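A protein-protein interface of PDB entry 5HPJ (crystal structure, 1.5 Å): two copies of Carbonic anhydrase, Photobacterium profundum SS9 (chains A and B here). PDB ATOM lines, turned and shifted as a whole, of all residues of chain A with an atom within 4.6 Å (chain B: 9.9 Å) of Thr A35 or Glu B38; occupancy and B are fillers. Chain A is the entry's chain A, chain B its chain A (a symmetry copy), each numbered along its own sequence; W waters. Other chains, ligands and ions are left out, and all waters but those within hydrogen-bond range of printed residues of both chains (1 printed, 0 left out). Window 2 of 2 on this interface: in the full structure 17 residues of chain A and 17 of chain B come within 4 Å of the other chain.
The backbone carbonyl oxygen (O) of Gln A36 is in hydrogen-bond range of the backbone NH (N) of Glu B38 (2.9 Å).
The guanidinium group of Arg B163 is in salt-bridge range of the side-chain carboxylate of Asp B73. The chain-end carboxylate of Glu B217 is in hydrogen-bond range of the backbone NH of Ala B37 (2.9 Å). The backbone carbonyl oxygen (O) of Leu B216 sits at hydrogen-bond distance from the backbone NH (N) of Arg B163. N of Glu A217 lies within hydrogen-bond range of O of Thr A35, 3.0 Å away. O of Ile B215 lies within hydrogen-bond range of N of Thr B35 (2.8 Å). O of Thr B35 is in hydrogen-bond range of N of Glu B217 (3.0 Å).
Ala B37 touches Thr A35. Glu B38 touches Thr A35. Gln A36 touches Ala B37 (O to CA, 3.3 Å). Thr B35 touches Ala A37 (CG2 to CB, 3.9 Å). Ala A37 touches Gln B36. Arg B163 touches Leu A214. Leu A214 touches Leu B216. Leu B214 touches Leu A216 (CD1 to CD1, 3.9 Å).
No residue of chain B comes within 4 Å of Thr A34. Thr A35 touches just these residues of chain B: Ala B37 (3.9 Å) and Glu B38 (3.8 Å). Gln A36 touches two residues of chain B. Ala A37 touches just these residues of chain B: Thr B35 (3.9 Å) and Gln B36 (3.3 Å). Printed residues of chain B within 4 Å of Leu A216: Leu B214. Of the printed residues of chain A, Gln B36 touches Ala A37 (3.3 Å). Of the printed residues of chain A, Ala B37 touches Thr A35 (3.9 Å) and Gln A36 (3.3 Å). Of chain A, only Thr A35 (3.8 Å) and Gln A36 (2.9 Å) come within 4 Å of Glu B38. Leu B39 touches none of the printed residues of chain A. Of the printed residues of chain A, Arg B163 touches Leu A214 (3.5 Å). Of the printed residues of chain A, Leu B216 touches Leu A214. The nearest residue of chain B that does not touch Thr A35 is Leu B39 (4.6 Å). The nearest printed residue of chain A that does not touch Glu B38 is Ala A37 (5.1 Å).
Hydrophobic or aromatic side chains of chain A within 4 Å of the printed part of chain B: Ala A37, Leu A214 and Leu A216. Of the 14 printed residues of chain B, 7 touch a printed residue of chain A. Hydrophobic or aromatic side chains of chain B within 4 Å of the printed part of chain A: Ala B37, Leu B214 and Leu B216. Along chain B the printed residues that touch a printed residue of chain A span positions 35 to 216. Among the printed residues, 9 pairs touch across the chains.
Thr A35 touches Ala B37, and with the chains exchanged Ala A37 touches Thr B35. Gln A36 touches Ala B37, and with the chains exchanged Ala A37 touches Gln B36. Leu A214 touches Leu B216, and with the chains exchanged Leu A216 touches Leu B214. Positions printed for both chains: 35, 36, 37, 214, 215, 216 and 217. Of the 9 pairs that touch across the chains among the printed residues, 6 have their exchanged pair printed and touching as well.
Water W1 lies within hydrogen-bond range of N of Gln A36 (3.0 Å) and O of Glu B38 (3.2 Å).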
ATOM      1  N   THR A  34     -32.281  18.904   4.113  1.00  0.00           N
ATOM      2  CA  THR A  34     -30.909  19.191   3.725  1.00  0.00           C
ATOM      3  C   THR A  34     -30.241  17.991   3.083  1.00  0.00           C
ATOM      4  O   THR A  34     -30.679  16.853   3.256  1.00  0.00           O
ATOM      5  CB  THR A  34     -30.052  19.605   4.919  1.00  0.00           C
ATOM      6  OG1 THR A  34     -29.984  18.508   5.835  1.00  0.00           O
ATOM      7  CG2 THR A  34     -30.639  20.841   5.604  1.00  0.00           C
ATOM      8  N   THR A  35     -29.156  18.282   2.382  1.00  0.00           N
ATOM      9  CA  THR A  35     -28.325  17.306   1.708  1.00  0.00           C
ATOM     10  C   THR A  35     -26.979  17.221   2.418  1.00  0.00           C
ATOM     11  O   THR A  35     -26.306  18.235   2.649  1.00  0.00           O
ATOM     12  CB  THR A  35     -28.147  17.712   0.241  1.00  0.00           C
ATOM     13  OG1 THR A  35     -29.404  17.582  -0.442  1.00  0.00           O
ATOM     14  CG2 THR A  35     -27.101  16.845  -0.475  1.00  0.00           C
ATOM     15  N   GLN A  36     -26.583  16.002   2.766  1.00  0.00           N
ATOM     16  CA  GLN A  36     -25.299  15.761   3.397  1.00  0.00           C
ATOM     17  C   GLN A  36     -24.211  15.924   2.360  1.00  0.00           C
ATOM     18  O   GLN A  36     -24.257  15.310   1.281  1.00  0.00           O
ATOM     19  CB  GLN A  36     -25.248  14.359   3.993  1.00  0.00           C
ATOM     20  CG  GLN A  36     -26.332  14.076   5.017  1.00  0.00           C
ATOM     21  CD  GLN A  36     -26.180  14.906   6.273  1.00  0.00           C
ATOM     22  OE1 GLN A  36     -25.087  15.023   6.819  1.00  0.00           O
ATOM     23  NE2 GLN A  36     -27.283  15.488   6.739  1.00  0.00           N
ATOM     24  N   ALA A  37     -23.232  16.760   2.671  1.00  0.00           N
ATOM     25  CA  ALA A  37     -22.145  17.065   1.758  1.00  0.00           C
ATOM     26  C   ALA A  37     -20.823  17.200   2.498  1.00  0.00           C
ATOM     27  O   ALA A  37     -20.794  17.440   3.714  1.00  0.00           O
ATOM     28  CB  ALA A  37     -22.444  18.323   0.984  1.00  0.00           C
ATOM     29  N   LEU A 214     -30.367  23.274  -3.322  1.00  0.00           N
ATOM     30  CA  LEU A 214     -30.298  22.377  -2.173  1.00  0.00           C
ATOM     31  C   LEU A 214     -29.487  23.039  -1.058  1.00  0.00           C
ATOM     32  O   LEU A 214     -28.523  23.794  -1.310  1.00  0.00           O
ATOM     33  CB  LEU A 214     -29.657  21.047  -2.544  1.00  0.00           C
ATOM     34  CG  LEU A 214     -30.418  20.190  -3.562  1.00  0.00           C
ATOM     35  CD1 LEU A 214     -29.598  18.944  -3.873  1.00  0.00           C
ATOM     36  CD2 LEU A 214     -31.798  19.805  -3.086  1.00  0.00           C
ATOM     37  N   ILE A 215     -29.902  22.784   0.171  1.00  0.00           N
ATOM     38  CA  ILE A 215     -29.198  23.254   1.352  1.00  0.00           C
ATOM     39  C   ILE A 215     -28.266  22.143   1.794  1.00  0.00           C
ATOM     40  O   ILE A 215     -28.662  20.985   1.873  1.00  0.00           O
ATOM     41  CB  ILE A 215     -30.156  23.557   2.511  1.00  0.00           C
ATOM     42  CG1 ILE A 215     -31.318  24.450   2.054  1.00  0.00           C
ATOM     43  CG2 ILE A 215     -29.354  24.174   3.662  1.00  0.00           C
ATOM     44  CD1 ILE A 215     -32.478  24.470   3.046  1.00  0.00           C
ATOM     45  N   LEU A 216     -27.022  22.500   2.072  1.00  0.00           N
ATOM     46  CA  LEU A 216     -25.986  21.539   2.377  1.00  0.00           C
ATOM     47  C   LEU A 216     -25.622  21.576   3.849  1.00  0.00           C
ATOM     48  O   LEU A 216     -25.616  22.638   4.476  1.00  0.00           O
ATOM     49  CB  LEU A 216     -24.732  21.847   1.577  1.00  0.00           C
ATOM     50  CG  LEU A 216     -24.943  21.998   0.068  1.00  0.00           C
ATOM     51  CD1 LEU A 216     -23.617  22.310  -0.615  1.00  0.00           C
ATOM     52  CD2 LEU A 216     -25.571  20.744  -0.507  1.00  0.00           C
ATOM     53  N   GLU A 217     -25.276  20.418   4.393  1.00  0.00           N
ATOM     54  CA  GLU A 217     -24.703  20.370   5.729  1.00  0.00           C
ATOM     55  C   GLU A 217     -23.686  19.258   5.849  1.00  0.00           C
ATOM     56  O   GLU A 217     -22.875  19.279   6.795  1.00  0.00           O
ATOM     57  CB  GLU A 217     -25.776  20.214   6.778  1.00  0.00           C
ATOM     58  CG  GLU A 217     -26.473  18.890   6.775  1.00  0.00           C
ATOM     59  CD  GLU A 217     -27.305  18.690   8.032  1.00  0.00           C
ATOM     60  OE1 GLU A 217     -28.541  18.769   7.970  1.00  0.00           O
ATOM     61  OE2 GLU A 217     -26.704  18.462   9.109  1.00  0.00           O
ATOM     62  OXT GLU A 217     -23.652  18.358   5.006  1.00  0.00           O
ATOM     63  N   THR B  35     -18.333  19.241  -5.161  1.00  0.00           N
ATOM     64  CA  THR B  35     -18.553  18.845  -3.785  1.00  0.00           C
ATOM     65  C   THR B  35     -19.260  17.496  -3.762  1.00  0.00           C
ATOM     66  O   THR B  35     -20.297  17.298  -4.411  1.00  0.00           O
ATOM     67  CB  THR B  35     -19.389  19.915  -3.073  1.00  0.00           C
ATOM     68  OG1 THR B  35     -18.606  21.112  -2.937  1.00  0.00           O
ATOM     69  CG2 THR B  35     -19.845  19.458  -1.681  1.00  0.00           C
ATOM     70  N   GLN B  36     -18.697  16.558  -3.007  1.00  0.00           N
ATOM     71  CA  GLN B  36     -19.289  15.245  -2.842  1.00  0.00           C
ATOM     72  C   GLN B  36     -20.504  15.368  -1.952  1.00  0.00           C
ATOM     73  O   GLN B  36     -20.433  15.924  -0.844  1.00  0.00           O
ATOM     74  CB  GLN B  36     -18.286  14.276  -2.226  1.00  0.00           C
ATOM     75  CG  GLN B  36     -17.004  14.115  -3.023  1.00  0.00           C
ATOM     76  CD  GLN B  36     -17.229  13.449  -4.363  1.00  0.00           C
ATOM     77  OE1 GLN B  36     -17.926  12.444  -4.454  1.00  0.00           O
ATOM     78  NE2 GLN B  36     -16.635  14.010  -5.414  1.00  0.00           N
ATOM     79  N   ALA B  37     -21.630  14.863  -2.433  1.00  0.00           N
ATOM     80  CA  ALA B  37     -22.894  14.952  -1.721  1.00  0.00           C
ATOM     81  C   ALA B  37     -23.709  13.678  -1.878  1.00  0.00           C
ATOM     82  O   ALA B  37     -23.497  12.896  -2.817  1.00  0.00           O
ATOM     83  CB  ALA B  37     -23.684  16.143  -2.200  1.00  0.00           C
ATOM     84  N   GLU B  38     -24.629  13.478  -0.948  1.00  0.00           N
ATOM     85  CA  GLU B  38     -25.526  12.329  -0.980  1.00  0.00           C
ATOM     86  C   GLU B  38     -26.789  12.662  -1.749  1.00  0.00           C
ATOM     87  O   GLU B  38     -27.755  13.172  -1.179  1.00  0.00           O
ATOM     88  CB  GLU B  38     -25.830  11.874   0.439  1.00  0.00           C
ATOM     89  CG  GLU B  38     -24.551  11.461   1.174  1.00  0.00           C
ATOM     90  CD  GLU B  38     -24.789  10.881   2.560  1.00  0.00           C
ATOM     91  OE1 GLU B  38     -25.952  10.821   2.997  1.00  0.00           O
ATOM     92  OE2 GLU B  38     -23.801  10.484   3.212  1.00  0.00           O
ATOM     93  N   LEU B  39     -26.768  12.325  -3.040  1.00  0.00           N
ATOM     94  CA  LEU B  39     -27.810  12.689  -4.002  1.00  0.00           C
ATOM     95  C   LEU B  39     -28.637  11.470  -4.396  1.00  0.00           C
ATOM     96  O   LEU B  39     -28.091  10.395  -4.626  1.00  0.00           O
ATOM     97  CB  LEU B  39     -27.152  13.222  -5.276  1.00  0.00           C
ATOM     98  CG  LEU B  39     -26.255  14.465  -5.163  1.00  0.00           C
ATOM     99  CD1 LEU B  39     -25.400  14.622  -6.421  1.00  0.00           C
ATOM    100  CD2 LEU B  39     -27.097  15.672  -4.916  1.00  0.00           C
ATOM    101  N   ALA B  40     -29.945  11.653  -4.512  1.00  0.00           N
ATOM    102  CA  ALA B  40     -30.844  10.577  -4.905  1.00  0.00           C
ATOM    103  C   ALA B  40     -30.657  10.228  -6.370  1.00  0.00           C
ATOM    104  O   ALA B  40     -30.383  11.096  -7.188  1.00  0.00           O
ATOM    105  CB  ALA B  40     -32.290  11.004  -4.682  1.00  0.00           C
ATOM    106  N   PRO B  41     -30.833   8.955  -6.728  1.00  0.00           N
ATOM    107  CA  PRO B  41     -30.828   8.657  -8.166  1.00  0.00           C
ATOM    108  C   PRO B  41     -31.972   9.334  -8.906  1.00  0.00           C
ATOM    109  O   PRO B  41     -33.068   9.454  -8.357  1.00  0.00           O
ATOM    110  CB  PRO B  41     -31.011   7.136  -8.206  1.00  0.00           C
ATOM    111  CG  PRO B  41     -30.619   6.660  -6.853  1.00  0.00           C
ATOM    112  CD  PRO B  41     -31.033   7.747  -5.914  1.00  0.00           C
ATOM    113  N   ASP B  73     -36.811  15.225  -6.508  1.00  0.00           N
ATOM    114  CA  ASP B  73     -37.179  16.240  -5.519  1.00  0.00           C
ATOM    115  C   ASP B  73     -38.677  16.221  -5.193  1.00  0.00           C
ATOM    116  O   ASP B  73     -39.219  17.222  -4.718  1.00  0.00           O
ATOM    117  CB  ASP B  73     -36.767  17.643  -5.954  1.00  0.00           C
ATOM    118  CG  ASP B  73     -35.255  17.851  -5.983  1.00  0.00           C
ATOM    119  OD1 ASP B  73     -34.494  17.061  -5.390  1.00  0.00           O
ATOM    120  OD2 ASP B  73     -34.841  18.865  -6.588  1.00  0.00           O
ATOM    121  N   TYR B 161     -24.783  11.677 -12.099  1.00  0.00           N
ATOM    122  CA  TYR B 161     -24.877  13.031 -12.611  1.00  0.00           C
ATOM    123  C   TYR B 161     -24.200  14.045 -11.697  1.00  0.00           C
ATOM    124  O   TYR B 161     -23.936  13.776 -10.521  1.00  0.00           O
ATOM    125  CB  TYR B 161     -26.346  13.414 -12.768  1.00  0.00           C
ATOM    126  CG  TYR B 161     -27.137  13.385 -11.472  1.00  0.00           C
ATOM    127  CD1 TYR B 161     -27.798  12.238 -11.068  1.00  0.00           C
ATOM    128  CD2 TYR B 161     -27.250  14.510 -10.679  1.00  0.00           C
ATOM    129  CE1 TYR B 161     -28.545  12.205  -9.888  1.00  0.00           C
ATOM    130  CE2 TYR B 161     -27.980  14.489  -9.494  1.00  0.00           C
ATOM    131  CZ  TYR B 161     -28.642  13.339  -9.106  1.00  0.00           C
ATOM    132  OH  TYR B 161     -29.370  13.344  -7.943  1.00  0.00           O
ATOM    133  N   ARG B 163     -25.064  17.853 -10.245  1.00  0.00           N
ATOM    134  CA  ARG B 163     -26.221  18.705 -10.061  1.00  0.00           C
ATOM    135  C   ARG B 163     -25.831  20.125  -9.723  1.00  0.00           C
ATOM    136  O   ARG B 163     -24.978  20.388  -8.872  1.00  0.00           O
ATOM    137  CB  ARG B 163     -27.137  18.169  -8.959  1.00  0.00           C
ATOM    138  CG  ARG B 163     -28.311  19.111  -8.673  1.00  0.00           C
ATOM    139  CD  ARG B 163     -29.214  18.631  -7.555  1.00  0.00           C
ATOM    140  NE  ARG B 163     -30.246  19.629  -7.285  1.00  0.00           N
ATOM    141  CZ  ARG B 163     -31.501  19.355  -6.950  1.00  0.00           C
ATOM    142  NH1 ARG B 163     -31.908  18.099  -6.830  1.00  0.00           N
ATOM    143  NH2 ARG B 163     -32.353  20.350  -6.729  1.00  0.00           N
ATOM    144  N   LEU B 214     -22.274  25.825  -5.378  1.00  0.00           N
ATOM    145  CA  LEU B 214     -21.418  24.645  -5.465  1.00  0.00           C
ATOM    146  C   LEU B 214     -22.066  23.615  -6.391  1.00  0.00           C
ATOM    147  O   LEU B 214     -23.307  23.483  -6.457  1.00  0.00           O
ATOM    148  CB  LEU B 214     -21.191  24.022  -4.094  1.00  0.00           C
ATOM    149  CG  LEU B 214     -20.431  24.882  -3.078  1.00  0.00           C
ATOM    150  CD1 LEU B 214     -20.365  24.139  -1.750  1.00  0.00           C
ATOM    151  CD2 LEU B 214     -19.042  25.248  -3.544  1.00  0.00           C
ATOM    152  N   ILE B 215     -21.225  22.911  -7.130  1.00  0.00           N
ATOM    153  CA  ILE B 215     -21.655  21.828  -7.997  1.00  0.00           C
ATOM    154  C   ILE B 215     -21.520  20.539  -7.212  1.00  0.00           C
ATOM    155  O   ILE B 215     -20.500  20.297  -6.575  1.00  0.00           O
ATOM    156  CB  ILE B 215     -20.781  21.713  -9.253  1.00  0.00           C
ATOM    157  CG1 ILE B 215     -20.621  23.072  -9.947  1.00  0.00           C
ATOM    158  CG2 ILE B 215     -21.382  20.646 -10.173  1.00  0.00           C
ATOM    159  CD1 ILE B 215     -19.478  23.092 -10.961  1.00  0.00           C
ATOM    160  N   LEU B 216     -22.557  19.719  -7.253  1.00  0.00           N
ATOM    161  CA  LEU B 216     -22.630  18.518  -6.452  1.00  0.00           C
ATOM    162  C   LEU B 216     -22.459  17.277  -7.308  1.00  0.00           C
ATOM    163  O   LEU B 216     -22.915  17.227  -8.453  1.00  0.00           O
ATOM    164  CB  LEU B 216     -23.981  18.427  -5.764  1.00  0.00           C
ATOM    165  CG  LEU B 216     -24.390  19.669  -4.967  1.00  0.00           C
ATOM    166  CD1 LEU B 216     -25.760  19.454  -4.333  1.00  0.00           C
ATOM    167  CD2 LEU B 216     -23.348  19.991  -3.914  1.00  0.00           C
ATOM    168  N   GLU B 217     -21.834  16.256  -6.738  1.00  0.00           N
ATOM    169  CA  GLU B 217     -21.807  14.952  -7.383  1.00  0.00           C
ATOM    170  C   GLU B 217     -21.833  13.837  -6.363  1.00  0.00           C
ATOM    171  O   GLU B 217     -22.140  12.687  -6.732  1.00  0.00           O
ATOM    172  CB  GLU B 217     -20.603  14.814  -8.281  1.00  0.00           C
ATOM    173  CG  GLU B 217     -19.288  14.751  -7.568  1.00  0.00           C
ATOM    174  CD  GLU B 217     -18.168  14.304  -8.494  1.00  0.00           C
ATOM    175  OE1 GLU B 217     -17.335  15.129  -8.895  1.00  0.00           O
ATOM    176  OE2 GLU B 217     -18.130  13.098  -8.838  1.00  0.00           O
ATOM    177  OXT GLU B 217     -21.571  14.074  -5.182  1.00  0.00           O
HETATM  178  O   HOH W   1     -28.398  13.734   1.912  1.00  0.00           O
